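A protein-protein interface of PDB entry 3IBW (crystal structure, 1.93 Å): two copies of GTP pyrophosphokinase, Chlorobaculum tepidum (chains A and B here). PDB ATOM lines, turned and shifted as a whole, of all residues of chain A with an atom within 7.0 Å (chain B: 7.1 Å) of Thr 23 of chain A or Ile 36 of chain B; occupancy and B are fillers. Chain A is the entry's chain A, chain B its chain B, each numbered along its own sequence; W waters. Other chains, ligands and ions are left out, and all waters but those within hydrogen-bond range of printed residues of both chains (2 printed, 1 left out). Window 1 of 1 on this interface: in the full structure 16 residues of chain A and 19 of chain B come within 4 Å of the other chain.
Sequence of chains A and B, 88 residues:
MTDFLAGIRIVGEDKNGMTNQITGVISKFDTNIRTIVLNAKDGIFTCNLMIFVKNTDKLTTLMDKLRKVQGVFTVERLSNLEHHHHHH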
ATOM      1  N   GLY A  17     -12.941   5.416 -16.166  1.00  0.00           N
ATOM      2  CA  GLY A  17     -13.026   3.977 -16.335  1.00  0.00           C
ATOM      3  C   GLY A  17     -14.312   3.448 -16.956  1.00  0.00           C
ATOM      4  O   GLY A  17     -14.679   2.291 -16.749  1.00  0.00           O
ATOM      5  N   MET A  18     -14.993   4.284 -17.732  1.00  0.00           N
ATOM      6  CA  MET A  18     -16.252   3.885 -18.360  1.00  0.00           C
ATOM      7  C   MET A  18     -16.186   2.726 -19.361  1.00  0.00           C
ATOM      8  O   MET A  18     -17.098   1.898 -19.402  1.00  0.00           O
ATOM      9  CB  MET A  18     -16.896   5.092 -19.045  1.00  0.00           C
ATOM     10  CG  MET A  18     -17.622   6.051 -18.111  1.00  0.00           C
ATOM     11  SD  MET A  18     -19.111   5.202 -17.208  1.00  0.00           S
ATOM     12  CE  MET A  18     -19.788   4.112 -18.649  1.00  0.00           C
ATOM     13  N   THR A  19     -15.127   2.655 -20.167  1.00  0.00           N
ATOM     14  CA  THR A  19     -15.026   1.572 -21.145  1.00  0.00           C
ATOM     15  C   THR A  19     -14.899   0.244 -20.400  1.00  0.00           C
ATOM     16  O   THR A  19     -15.532  -0.746 -20.769  1.00  0.00           O
ATOM     17  CB  THR A  19     -13.846   1.793 -22.122  1.00  0.00           C
ATOM     18  OG1 THR A  19     -12.650   2.053 -21.379  1.00  0.00           O
ATOM     19  CG2 THR A  19     -14.148   2.976 -23.059  1.00  0.00           C
ATOM     20  N   ASN A  20     -14.084   0.220 -19.350  1.00  0.00           N
ATOM     21  CA  ASN A  20     -13.944  -0.990 -18.542  1.00  0.00           C
ATOM     22  C   ASN A  20     -15.272  -1.285 -17.832  1.00  0.00           C
ATOM     23  O   ASN A  20     -15.679  -2.444 -17.723  1.00  0.00           O
ATOM     24  CB  ASN A  20     -12.848  -0.822 -17.485  1.00  0.00           C
ATOM     25  CG  ASN A  20     -11.459  -1.023 -18.048  1.00  0.00           C
ATOM     26  OD1 ASN A  20     -10.730  -1.928 -17.632  1.00  0.00           O
ATOM     27  ND2 ASN A  20     -11.088  -0.190 -19.008  1.00  0.00           N
ATOM     28  N   GLN A  21     -15.951  -0.249 -17.342  1.00  0.00           N
ATOM     29  CA  GLN A  21     -17.222  -0.468 -16.655  1.00  0.00           C
ATOM     30  C   GLN A  21     -18.272  -1.084 -17.574  1.00  0.00           C
ATOM     31  O   GLN A  21     -18.953  -2.037 -17.189  1.00  0.00           O
ATOM     32  CB  GLN A  21     -17.767   0.843 -16.060  1.00  0.00           C
ATOM     33  CG  GLN A  21     -19.200   0.719 -15.536  1.00  0.00           C
ATOM     34  CD  GLN A  21     -19.553   1.763 -14.489  1.00  0.00           C
ATOM     35  OE1 GLN A  21     -18.956   2.836 -14.439  1.00  0.00           O
ATOM     36  NE2 GLN A  21     -20.539   1.450 -13.652  1.00  0.00           N
ATOM     37  N   ILE A  22     -18.394  -0.557 -18.791  1.00  0.00           N
ATOM     38  CA  ILE A  22     -19.390  -1.064 -19.728  1.00  0.00           C
ATOM     39  C   ILE A  22     -19.072  -2.476 -20.197  1.00  0.00           C
ATOM     40  O   ILE A  22     -19.970  -3.300 -20.384  1.00  0.00           O
ATOM     41  CB  ILE A  22     -19.547  -0.114 -20.947  1.00  0.00           C
ATOM     42  CG1 ILE A  22     -20.405   1.095 -20.552  1.00  0.00           C
ATOM     43  CG2 ILE A  22     -20.205  -0.843 -22.103  1.00  0.00           C
ATOM     44  CD1 ILE A  22     -21.784   0.727 -20.018  1.00  0.00           C
ATOM     45  N   THR A  23     -17.789  -2.752 -20.381  1.00  0.00           N
ATOM     46  CA  THR A  23     -17.373  -4.074 -20.809  1.00  0.00           C
ATOM     47  C   THR A  23     -17.696  -5.067 -19.681  1.00  0.00           C
ATOM     48  O   THR A  23     -18.084  -6.202 -19.944  1.00  0.00           O
ATOM     49  CB  THR A  23     -15.867  -4.099 -21.147  1.00  0.00           C
ATOM     50  OG1 THR A  23     -15.607  -3.190 -22.230  1.00  0.00           O
ATOM     51  CG2 THR A  23     -15.439  -5.499 -21.571  1.00  0.00           C
ATOM     52  N   GLY A  24     -17.552  -4.628 -18.430  1.00  0.00           N
ATOM     53  CA  GLY A  24     -17.857  -5.491 -17.297  1.00  0.00           C
ATOM     54  C   GLY A  24     -19.340  -5.834 -17.207  1.00  0.00           C
ATOM     55  O   GLY A  24     -19.706  -6.974 -16.914  1.00  0.00           O
ATOM     56  N   VAL A  25     -20.195  -4.843 -17.454  1.00  0.00           N
ATOM     57  CA  VAL A  25     -21.648  -5.024 -17.425  1.00  0.00           C
ATOM     58  C   VAL A  25     -22.053  -6.037 -18.488  1.00  0.00           C
ATOM     59  O   VAL A  25     -22.874  -6.926 -18.243  1.00  0.00           O
ATOM     60  CB  VAL A  25     -22.380  -3.687 -17.720  1.00  0.00           C
ATOM     61  CG1 VAL A  25     -23.870  -3.937 -17.939  1.00  0.00           C
ATOM     62  CG2 VAL A  25     -22.169  -2.718 -16.567  1.00  0.00           C
ATOM     63  N   ILE A  26     -21.474  -5.893 -19.673  1.00  0.00           N
ATOM     64  CA  ILE A  26     -21.763  -6.792 -20.787  1.00  0.00           C
ATOM     65  C   ILE A  26     -21.321  -8.227 -20.472  1.00  0.00           C
ATOM     66  O   ILE A  26     -22.047  -9.181 -20.745  1.00  0.00           O
ATOM     67  CB  ILE A  26     -21.049  -6.314 -22.072  1.00  0.00           C
ATOM     68  CG1 ILE A  26     -21.687  -5.010 -22.562  1.00  0.00           C
ATOM     69  CG2 ILE A  26     -21.127  -7.393 -23.154  1.00  0.00           C
ATOM     70  CD1 ILE A  26     -20.905  -4.323 -23.660  1.00  0.00           C
ATOM     71  N   SER A  27     -20.134  -8.374 -19.889  1.00  0.00           N
ATOM     72  CA  SER A  27     -19.621  -9.697 -19.560  1.00  0.00           C
ATOM     73  C   SER A  27     -20.531 -10.404 -18.555  1.00  0.00           C
ATOM     74  O   SER A  27     -20.717 -11.619 -18.629  1.00  0.00           O
ATOM     75  CB  SER A  27     -18.187  -9.595 -19.011  1.00  0.00           C
ATOM     76  OG  SER A  27     -18.145  -8.991 -17.732  1.00  0.00           O
ATOM     77  N   LYS A  28     -21.110  -9.641 -17.629  1.00  0.00           N
ATOM     78  CA  LYS A  28     -21.991 -10.218 -16.620  1.00  0.00           C
ATOM     79  C   LYS A  28     -23.375 -10.598 -17.149  1.00  0.00           C
ATOM     80  O   LYS A  28     -24.145 -11.275 -16.468  1.00  0.00           O
ATOM     81  CB  LYS A  28     -22.069  -9.290 -15.402  1.00  0.00           C
ATOM     82  CG  LYS A  28     -20.770  -9.301 -14.592  1.00  0.00           C
ATOM     83  CD  LYS A  28     -20.791  -8.274 -13.471  1.00  0.00           C
ATOM     84  CE  LYS A  28     -19.401  -8.113 -12.866  1.00  0.00           C
ATOM     85  NZ  LYS A  28     -19.220  -6.804 -12.171  1.00  0.00           N
ATOM     86  N   ILE A  33     -22.549 -13.776 -26.473  1.00  0.00           N
ATOM     87  CA  ILE A  33     -22.049 -12.622 -27.213  1.00  0.00           C
ATOM     88  C   ILE A  33     -21.461 -13.071 -28.540  1.00  0.00           C
ATOM     89  O   ILE A  33     -20.660 -14.008 -28.590  1.00  0.00           O
ATOM     90  CB  ILE A  33     -20.972 -11.859 -26.386  1.00  0.00           C
ATOM     91  CG1 ILE A  33     -21.603 -11.313 -25.098  1.00  0.00           C
ATOM     92  CG2 ILE A  33     -20.364 -10.730 -27.223  1.00  0.00           C
ATOM     93  CD1 ILE A  33     -20.579 -10.910 -24.041  1.00  0.00           C
ATOM     94  N   ILE A  36     -18.436  -7.625 -30.601  1.00  0.00           N
ATOM     95  CA  ILE A  36     -18.314  -6.389 -29.844  1.00  0.00           C
ATOM     96  C   ILE A  36     -17.361  -5.507 -30.637  1.00  0.00           C
ATOM     97  O   ILE A  36     -16.256  -5.939 -30.985  1.00  0.00           O
ATOM     98  CB  ILE A  36     -17.703  -6.544 -28.430  1.00  0.00           C
ATOM     99  CG1 ILE A  36     -18.663  -7.308 -27.522  1.00  0.00           C
ATOM    100  CG2 ILE A  36     -17.396  -5.139 -27.848  1.00  0.00           C
ATOM    101  CD1 ILE A  36     -18.059  -7.666 -26.164  1.00  0.00           C
ATOM    102  N   VAL A  37     -17.801  -4.298 -30.973  1.00  0.00           N
ATOM    103  CA  VAL A  37     -16.933  -3.335 -31.643  1.00  0.00           C
ATOM    104  C   VAL A  37     -17.030  -2.084 -30.767  1.00  0.00           C
ATOM    105  O   VAL A  37     -18.033  -1.367 -30.795  1.00  0.00           O
ATOM    106  CB  VAL A  37     -17.369  -3.003 -33.074  1.00  0.00           C
ATOM    107  CG1 VAL A  37     -16.476  -1.879 -33.625  1.00  0.00           C
ATOM    108  CG2 VAL A  37     -17.247  -4.258 -33.945  1.00  0.00           C
ATOM    109  N   LEU A  38     -15.988  -1.837 -29.977  1.00  0.00           N
ATOM    110  CA  LEU A  38     -15.940  -0.687 -29.076  1.00  0.00           C
ATOM    111  C   LEU A  38     -14.768   0.202 -29.455  1.00  0.00           C
ATOM    112  O   LEU A  38     -13.678  -0.286 -29.766  1.00  0.00           O
ATOM    113  CB  LEU A  38     -15.798  -1.156 -27.617  1.00  0.00           C
ATOM    114  CG  LEU A  38     -15.756  -0.068 -26.530  1.00  0.00           C
ATOM    115  CD1 LEU A  38     -16.319  -0.614 -25.231  1.00  0.00           C
ATOM    116  CD2 LEU A  38     -14.326   0.438 -26.334  1.00  0.00           C
ATOM    117  N   ASN A  39     -15.000   1.507 -29.431  1.00  0.00           N
ATOM    118  CA  ASN A  39     -13.957   2.461 -29.773  1.00  0.00           C
ATOM    119  C   ASN A  39     -14.133   3.697 -28.915  1.00  0.00           C
ATOM    120  O   ASN A  39     -15.246   4.190 -28.766  1.00  0.00           O
ATOM    121  CB  ASN A  39     -14.054   2.840 -31.250  1.00  0.00           C
ATOM    122  CG  ASN A  39     -12.753   2.634 -31.979  1.00  0.00           C
ATOM    123  OD1 ASN A  39     -11.754   3.295 -31.687  1.00  0.00           O
ATOM    124  ND2 ASN A  39     -12.750   1.711 -32.932  1.00  0.00           N
ATOM    125  N   ALA A  40     -13.042   4.189 -28.340  1.00  0.00           N
ATOM    126  CA  ALA A  40     -13.101   5.389 -27.513  1.00  0.00           C
ATOM    127  C   ALA A  40     -12.327   6.468 -28.265  1.00  0.00           C
ATOM    128  O   ALA A  40     -11.155   6.283 -28.600  1.00  0.00           O
ATOM    129  CB  ALA A  40     -12.479   5.123 -26.154  1.00  0.00           C
ATOM    130  N   CYS A  47     -20.143   1.621 -28.688  1.00  0.00           N
ATOM    131  CA  CYS A  47     -20.040   0.176 -28.589  1.00  0.00           C
ATOM    132  C   CYS A  47     -21.213  -0.490 -29.282  1.00  0.00           C
ATOM    133  O   CYS A  47     -22.359  -0.260 -28.899  1.00  0.00           O
ATOM    134  CB  CYS A  47     -20.033  -0.258 -27.121  1.00  0.00           C
ATOM    135  SG  CYS A  47     -19.848  -2.044 -26.890  1.00  0.00           S
ATOM    136  N   ASN A  48     -20.929  -1.287 -30.309  1.00  0.00           N
ATOM    137  CA  ASN A  48     -21.964  -2.033 -31.020  1.00  0.00           C
ATOM    138  C   ASN A  48     -21.774  -3.477 -30.560  1.00  0.00           C
ATOM    139  O   ASN A  48     -20.695  -4.054 -30.705  1.00  0.00           O
ATOM    140  CB  ASN A  48     -21.794  -1.928 -32.536  1.00  0.00           C
ATOM    141  CG  ASN A  48     -22.293  -0.606 -33.088  1.00  0.00           C
ATOM    142  OD1 ASN A  48     -22.774   0.254 -32.348  1.00  0.00           O
ATOM    143  ND2 ASN A  48     -22.185  -0.441 -34.397  1.00  0.00           N
ATOM    144  N   LEU A  66     -27.797  -1.324 -19.095  1.00  0.00           N
ATOM    145  CA  LEU A  66     -26.764  -0.478 -19.684  1.00  0.00           C
ATOM    146  C   LEU A  66     -27.140   1.001 -19.624  1.00  0.00           C
ATOM    147  O   LEU A  66     -26.284   1.848 -19.375  1.00  0.00           O
ATOM    148  CB  LEU A  66     -26.536  -0.866 -21.144  1.00  0.00           C
ATOM    149  CG  LEU A  66     -25.827  -2.203 -21.381  1.00  0.00           C
ATOM    150  CD1 LEU A  66     -26.134  -2.717 -22.776  1.00  0.00           C
ATOM    151  CD2 LEU A  66     -24.327  -2.028 -21.186  1.00  0.00           C
ATOM    152  N   ASN B  20     -17.681 -14.198 -22.605  1.00  0.00           N
ATOM    153  CA  ASN B  20     -17.997 -13.587 -21.323  1.00  0.00           C
ATOM    154  C   ASN B  20     -16.789 -13.630 -20.398  1.00  0.00           C
ATOM    155  O   ASN B  20     -16.533 -12.683 -19.653  1.00  0.00           O
ATOM    156  CB  ASN B  20     -19.165 -14.318 -20.657  1.00  0.00           C
ATOM    157  CG  ASN B  20     -20.418 -14.315 -21.505  1.00  0.00           C
ATOM    158  OD1 ASN B  20     -21.032 -13.273 -21.732  1.00  0.00           O
ATOM    159  ND2 ASN B  20     -20.801 -15.489 -21.987  1.00  0.00           N
ATOM    160  N   ILE B  22     -13.546 -13.822 -21.336  1.00  0.00           N
ATOM    161  CA  ILE B  22     -12.530 -12.919 -21.874  1.00  0.00           C
ATOM    162  C   ILE B  22     -12.853 -11.457 -21.549  1.00  0.00           C
ATOM    163  O   ILE B  22     -11.993 -10.712 -21.080  1.00  0.00           O
ATOM    164  CB  ILE B  22     -12.410 -13.066 -23.413  1.00  0.00           C
ATOM    165  CG1 ILE B  22     -11.813 -14.432 -23.763  1.00  0.00           C
ATOM    166  CG2 ILE B  22     -11.562 -11.931 -23.985  1.00  0.00           C
ATOM    167  CD1 ILE B  22     -10.430 -14.679 -23.185  1.00  0.00           C
ATOM    168  N   THR B  23     -14.093 -11.046 -21.797  1.00  0.00           N
ATOM    169  CA  THR B  23     -14.488  -9.665 -21.525  1.00  0.00           C
ATOM    170  C   THR B  23     -14.438  -9.381 -20.026  1.00  0.00           C
ATOM    171  O   THR B  23     -14.114  -8.265 -19.613  1.00  0.00           O
ATOM    172  CB  THR B  23     -15.904  -9.365 -22.071  1.00  0.00           C
ATOM    173  OG1 THR B  23     -16.839 -10.287 -21.507  1.00  0.00           O
ATOM    174  CG2 THR B  23     -15.921  -9.490 -23.595  1.00  0.00           C
ATOM    175  N   GLY B  24     -14.750 -10.395 -19.221  1.00  0.00           N
ATOM    176  CA  GLY B  24     -14.714 -10.246 -17.776  1.00  0.00           C
ATOM    177  C   GLY B  24     -13.296  -9.982 -17.291  1.00  0.00           C
ATOM    178  O   GLY B  24     -13.066  -9.088 -16.473  1.00  0.00           O
ATOM    179  N   ILE B  26     -10.664  -8.825 -19.033  1.00  0.00           N
ATOM    180  CA  ILE B  26     -10.179  -7.541 -19.522  1.00  0.00           C
ATOM    181  C   ILE B  26     -10.768  -6.352 -18.779  1.00  0.00           C
ATOM    182  O   ILE B  26     -10.059  -5.404 -18.446  1.00  0.00           O
ATOM    183  CB  ILE B  26     -10.473  -7.375 -21.033  1.00  0.00           C
ATOM    184  CG1 ILE B  26      -9.719  -8.442 -21.836  1.00  0.00           C
ATOM    185  CG2 ILE B  26     -10.056  -5.981 -21.497  1.00  0.00           C
ATOM    186  CD1 ILE B  26     -10.239  -8.620 -23.255  1.00  0.00           C
ATOM    187  N   SER B  27     -12.065  -6.400 -18.505  1.00  0.00           N
ATOM    188  CA  SER B  27     -12.705  -5.292 -17.816  1.00  0.00           C
ATOM    189  C   SER B  27     -12.280  -5.152 -16.364  1.00  0.00           C
ATOM    190  O   SER B  27     -12.136  -4.036 -15.869  1.00  0.00           O
ATOM    191  CB  SER B  27     -14.224  -5.430 -17.881  1.00  0.00           C
ATOM    192  OG  SER B  27     -14.656  -6.603 -17.219  1.00  0.00           O
ATOM    193  N   LYS B  28     -12.071  -6.278 -15.687  1.00  0.00           N
ATOM    194  CA  LYS B  28     -11.683  -6.270 -14.280  1.00  0.00           C
ATOM    195  C   LYS B  28     -10.244  -5.854 -14.028  1.00  0.00           C
ATOM    196  O   LYS B  28      -9.907  -5.370 -12.947  1.00  0.00           O
ATOM    197  CB  LYS B  28     -11.890  -7.658 -13.656  1.00  0.00           C
ATOM    198  CG  LYS B  28     -13.331  -7.992 -13.282  1.00  0.00           C
ATOM    199  CD  LYS B  28     -13.430  -9.309 -12.509  1.00  0.00           C
ATOM    200  CE  LYS B  28     -14.855  -9.857 -12.516  1.00  0.00           C
ATOM    201  NZ  LYS B  28     -15.345 -10.114 -13.905  1.00  0.00           N
ATOM    202  N   ILE B  33      -9.275   0.325 -21.422  1.00  0.00           N
ATOM    203  CA  ILE B  33      -9.637  -0.184 -22.742  1.00  0.00           C
ATOM    204  C   ILE B  33      -9.874   0.955 -23.724  1.00  0.00           C
ATOM    205  O   ILE B  33     -10.630   1.883 -23.440  1.00  0.00           O
ATOM    206  CB  ILE B  33     -10.917  -1.051 -22.671  1.00  0.00           C
ATOM    207  CG1 ILE B  33     -10.660  -2.289 -21.802  1.00  0.00           C
ATOM    208  CG2 ILE B  33     -11.348  -1.460 -24.085  1.00  0.00           C
ATOM    209  CD1 ILE B  33     -11.932  -2.995 -21.366  1.00  0.00           C
ATOM    210  N   ARG B  34      -9.228   0.881 -24.883  1.00  0.00           N
ATOM    211  CA  ARG B  34      -9.386   1.912 -25.905  1.00  0.00           C
ATOM    212  C   ARG B  34     -10.216   1.422 -27.090  1.00  0.00           C
ATOM    213  O   ARG B  34     -11.047   2.159 -27.629  1.00  0.00           O
ATOM    214  CB  ARG B  34      -8.021   2.359 -26.422  1.00  0.00           C
ATOM    215  CG  ARG B  34      -7.106   2.980 -25.375  1.00  0.00           C
ATOM    216  CD  ARG B  34      -7.457   4.433 -25.113  1.00  0.00           C
ATOM    217  NE  ARG B  34      -8.497   4.560 -24.107  1.00  0.00           N
ATOM    218  CZ  ARG B  34      -9.387   5.544 -24.057  1.00  0.00           C
ATOM    219  NH1 ARG B  34      -9.371   6.521 -24.956  1.00  0.00           N
ATOM    220  NH2 ARG B  34     -10.301   5.542 -23.099  1.00  0.00           N
ATOM    221  N   THR B  35      -9.994   0.171 -27.481  1.00  0.00           N
ATOM    222  CA  THR B  35     -10.700  -0.404 -28.616  1.00  0.00           C
ATOM    223  C   THR B  35     -10.858  -1.907 -28.447  1.00  0.00           C
ATOM    224  O   THR B  35      -9.957  -2.573 -27.944  1.00  0.00           O
ATOM    225  CB  THR B  35      -9.898  -0.197 -29.931  1.00  0.00           C
ATOM    226  OG1 THR B  35      -9.426   1.153 -30.008  1.00  0.00           O
ATOM    227  CG2 THR B  35     -10.759  -0.493 -31.142  1.00  0.00           C
ATOM    228  N   ILE B  36     -12.009  -2.426 -28.856  1.00  0.00           N
ATOM    229  CA  ILE B  36     -12.253  -3.865 -28.818  1.00  0.00           C
ATOM    230  C   ILE B  36     -12.882  -4.262 -30.152  1.00  0.00           C
ATOM    231  O   ILE B  36     -13.857  -3.645 -30.586  1.00  0.00           O
ATOM    232  CB  ILE B  36     -13.271  -4.312 -27.716  1.00  0.00           C
ATOM    233  CG1 ILE B  36     -12.702  -4.072 -26.320  1.00  0.00           C
ATOM    234  CG2 ILE B  36     -13.617  -5.818 -27.899  1.00  0.00           C
ATOM    235  CD1 ILE B  36     -13.749  -4.229 -25.208  1.00  0.00           C
ATOM    236  N   VAL B  37     -12.302  -5.247 -30.832  1.00  0.00           N
ATOM    237  CA  VAL B  37     -12.905  -5.771 -32.060  1.00  0.00           C
ATOM    238  C   VAL B  37     -12.916  -7.281 -31.785  1.00  0.00           C
ATOM    239  O   VAL B  37     -11.914  -7.977 -31.978  1.00  0.00           O
ATOM    240  CB  VAL B  37     -12.105  -5.460 -33.328  1.00  0.00           C
ATOM    241  CG1 VAL B  37     -12.780  -6.146 -34.518  1.00  0.00           C
ATOM    242  CG2 VAL B  37     -12.065  -3.944 -33.545  1.00  0.00           C
ATOM    243  N   LEU B  38     -14.072  -7.768 -31.344  1.00  0.00           N
ATOM    244  CA  LEU B  38     -14.261  -9.158 -30.964  1.00  0.00           C
ATOM    245  C   LEU B  38     -15.338  -9.824 -31.804  1.00  0.00           C
ATOM    246  O   LEU B  38     -16.404  -9.254 -32.019  1.00  0.00           O
ATOM    247  CB  LEU B  38     -14.620  -9.177 -29.468  1.00  0.00           C
ATOM    248  CG  LEU B  38     -14.908 -10.476 -28.709  1.00  0.00           C
ATOM    249  CD1 LEU B  38     -14.617 -10.280 -27.222  1.00  0.00           C
ATOM    250  CD2 LEU B  38     -16.354 -10.893 -28.918  1.00  0.00           C
ATOM    251  N   ASN B  39     -15.051 -11.022 -32.296  1.00  0.00           N
ATOM    252  CA  ASN B  39     -16.027 -11.749 -33.096  1.00  0.00           C
ATOM    253  C   ASN B  39     -15.973 -13.225 -32.738  1.00  0.00           C
ATOM    254  O   ASN B  39     -14.894 -13.781 -32.551  1.00  0.00           O
ATOM    255  CB  ASN B  39     -15.754 -11.590 -34.598  1.00  0.00           C
ATOM    256  CG  ASN B  39     -15.926 -10.161 -35.085  1.00  0.00           C
ATOM    257  OD1 ASN B  39     -14.956  -9.415 -35.219  1.00  0.00           O
ATOM    258  ND2 ASN B  39     -17.169  -9.769 -35.340  1.00  0.00           N
ATOM    259  N   CYS B  47     -10.225 -11.707 -31.000  1.00  0.00           N
ATOM    260  CA  CYS B  47     -10.389 -10.421 -30.338  1.00  0.00           C
ATOM    261  C   CYS B  47      -9.111  -9.599 -30.377  1.00  0.00           C
ATOM    262  O   CYS B  47      -8.060 -10.062 -29.922  1.00  0.00           O
ATOM    263  CB  CYS B  47     -10.806 -10.609 -28.873  1.00  0.00           C
ATOM    264  SG  CYS B  47     -10.944  -9.054 -27.930  1.00  0.00           S
ATOM    265  N   ASN B  48      -9.198  -8.406 -30.963  1.00  0.00           N
ATOM    266  CA  ASN B  48      -8.076  -7.471 -31.007  1.00  0.00           C
ATOM    267  C   ASN B  48      -8.451  -6.386 -29.997  1.00  0.00           C
ATOM    268  O   ASN B  48      -9.516  -5.767 -30.089  1.00  0.00           O
ATOM    269  CB  ASN B  48      -7.901  -6.858 -32.396  1.00  0.00           C
ATOM    270  CG  ASN B  48      -7.225  -7.805 -33.361  1.00  0.00           C
ATOM    271  OD1 ASN B  48      -6.715  -8.853 -32.965  1.00  0.00           O
ATOM    272  ND2 ASN B  48      -7.222  -7.445 -34.634  1.00  0.00           N
ATOM    273  N   LEU B  49      -7.560  -6.158 -29.043  1.00  0.00           N
ATOM    274  CA  LEU B  49      -7.769  -5.202 -27.969  1.00  0.00           C
ATOM    275  C   LEU B  49      -6.677  -4.137 -27.965  1.00  0.00           C
ATOM    276  O   LEU B  49      -5.510  -4.464 -28.166  1.00  0.00           O
ATOM    277  CB  LEU B  49      -7.742  -5.976 -26.633  1.00  0.00           C
ATOM    278  CG  LEU B  49      -7.672  -5.243 -25.282  1.00  0.00           C
ATOM    279  CD1 LEU B  49      -9.003  -4.560 -25.004  1.00  0.00           C
ATOM    280  CD2 LEU B  49      -7.346  -6.232 -24.161  1.00  0.00           C
ATOM    281  N   MET B  50      -7.064  -2.872 -27.786  1.00  0.00           N
ATOM    282  CA  MET B  50      -6.091  -1.783 -27.666  1.00  0.00           C
ATOM    283  C   MET B  50      -6.363  -1.245 -26.258  1.00  0.00           C
ATOM    284  O   MET B  50      -7.499  -0.924 -25.907  1.00  0.00           O
ATOM    285  CB  MET B  50      -6.310  -0.676 -28.702  1.00  0.00           C
ATOM    286  CG  MET B  50      -6.076  -1.112 -30.133  1.00  0.00           C
ATOM    287  SD  MET B  50      -4.226  -1.555 -30.510  1.00  0.00           S
ATOM    288  CE  MET B  50      -3.338  -0.280 -29.374  1.00  0.00           C
ATOM    289  N   ILE B  51      -5.314  -1.140 -25.456  1.00  0.00           N
ATOM    290  CA  ILE B  51      -5.448  -0.688 -24.079  1.00  0.00           C
ATOM    291  C   ILE B  51      -4.318   0.254 -23.693  1.00  0.00           C
ATOM    292  O   ILE B  51      -3.260   0.225 -24.315  1.00  0.00           O
ATOM    293  CB  ILE B  51      -5.369  -1.913 -23.091  1.00  0.00           C
ATOM    294  CG1 ILE B  51      -4.121  -2.759 -23.404  1.00  0.00           C
ATOM    295  CG2 ILE B  51      -6.621  -2.791 -23.194  1.00  0.00           C
ATOM    296  CD1 ILE B  51      -3.900  -3.905 -22.442  1.00  0.00           C
HETATM  297  O   HOH W   1     -17.526 -10.923 -15.660  1.00  0.00           O
HETATM  298  O   HOH W   2     -20.770 -15.119 -25.033  1.00  0.00           O
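The side-chain hydroxyl of Thr 19 of chain A sits at hydrogen-bond distance from the backbone carbonyl oxygen of Ile 33 of chain B.
OD1 of Asn 20 of chain A lies close to O of Ser 27 of chain B, 3.1 Å away.
The side-chain amide nitrogen of Asn 20 of chain A sits close to the backbone NH of Ile 33 of chain B (3.1 Å).
The backbone carbonyl oxygen of Ile 36 of chain A lies within hydrogen-bond range of the backbone NH of Leu 38 of chain B, 2.9 Å away.
The backbone NH (N) of Leu 38 of chain A sits at hydrogen-bond distance from the backbone carbonyl oxygen (O) of Ile 36 of chain B, 2.9 Å away.
N of Ala 40 of chain A is in hydrogen-bond range of O of Arg 34 of chain B.
The backbone carbonyl oxygen of Ile 36 of chain B sits close to the backbone carbonyl oxygen of Ile 36 of chain A.
The side-chain hydroxyl of Ser 27 of chain A is in hydrogen-bond range of the backbone carbonyl oxygen of Gly 24 of chain A (2.7 Å).
OG of Ser 27 of chain B is in hydrogen-bond range of O of Gly 24 of chain B (3.0 Å).
The backbone carbonyl oxygen of Thr 35 of chain B lies within hydrogen-bond range of the backbone NH of Met 50 of chain B (2.9 Å).
The backbone NH (N) of Val 37 of chain B is in hydrogen-bond range of the backbone carbonyl oxygen (O) of Asn 48 of chain B, at 2.9 Å.
Asn 20 of chain A touches Ile 26 of chain B.
Thr 23 of chain A touches Ser 27 of chain B.
OG of Ser 27 of chain B touches CA of Gly 24 of chain A, at 3.4 Å.
Ser 27 of chain A touches Asn 20 of chain B.
Ser 27 of chain A touches Thr 23 of chain B (CB to OG1, 2.9 Å).
Gly 24 of chain B touches Ser 27 of chain A (N to CB, 3.5 Å).
Thr 23 of chain B touches Ile 36 of chain A (CG2 to CD1, 3.8 Å).
Ile 36 of chain B touches Val 37 of chain A.
Thr 35 of chain B touches Asn 39 of chain A.
Met 18 of chain A touches none of the printed residues of chain B.
Printed residues of chain A within 4 Å of Asn 20 of chain B: Ser 27 (3.5 Å) and Ile 33 (3.3 Å).
Printed residues of chain A within 4 Å of Ile 26 of chain B: Asn 20.
Of the printed residues of chain A, Ile 33 of chain B touches Thr 19 (2.9 Å), Asn 20 (3.1 Å) and Thr 23 (3.8 Å).
Of chain A, only Thr 23 (3.7 Å), Ile 36 (3.3 Å), Val 37 (3.3 Å) and Leu 38 (2.9 Å) come within 4 Å of Ile 36 of chain B.
The nearest residue of chain B that does not touch Thr 23 of chain A is Ile 26 of chain B (5.3 Å).
The nearest residue of chain A that does not touch Ile 36 of chain B is Asn 39 of chain A (5.0 Å).
The nearest printed residue of chain B that does not touch Asn 39 of chain A is Ile 36 of chain B (5.0 Å).
Hydrophobic or aromatic side chains of chain A that line the printed part of chain B: Ile 33, Ile 36, Leu 38 and Ala 40.
Hydrophobic or aromatic side chains of chain B within 4 Å of the printed part of chain A: Ile 33, Ile 36 and Leu 38.
Among the printed residues, no Asp or Glu carboxylate lies within 4 Å of a Lys or Arg side-chain nitrogen of the other chain.
Asn 20 of chain A touches Ile 26 of chain B, but with the chains exchanged Ile 26 of chain A does not touch Asn 20 of chain B (4.3 Å).
Thr 23 of chain A touches Ile 33 of chain B, but with the chains exchanged Ile 33 of chain A does not touch Thr 23 of chain B (4.6 Å).
Ile 36 of chain A touches Leu 38 of chain B, and with the chains exchanged Leu 38 of chain A touches Ile 36 of chain B.
Water W2 bridges the backbone NH (N) of Ile 33 of chain A and the side-chain amide nitrogen (ND2) of Asn 20 of chain B.
Water W1 lies within hydrogen-bond range of OG of Ser 27 of chain A (2.9 Å) and NZ of Lys 28 of chain B (2.9 Å).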
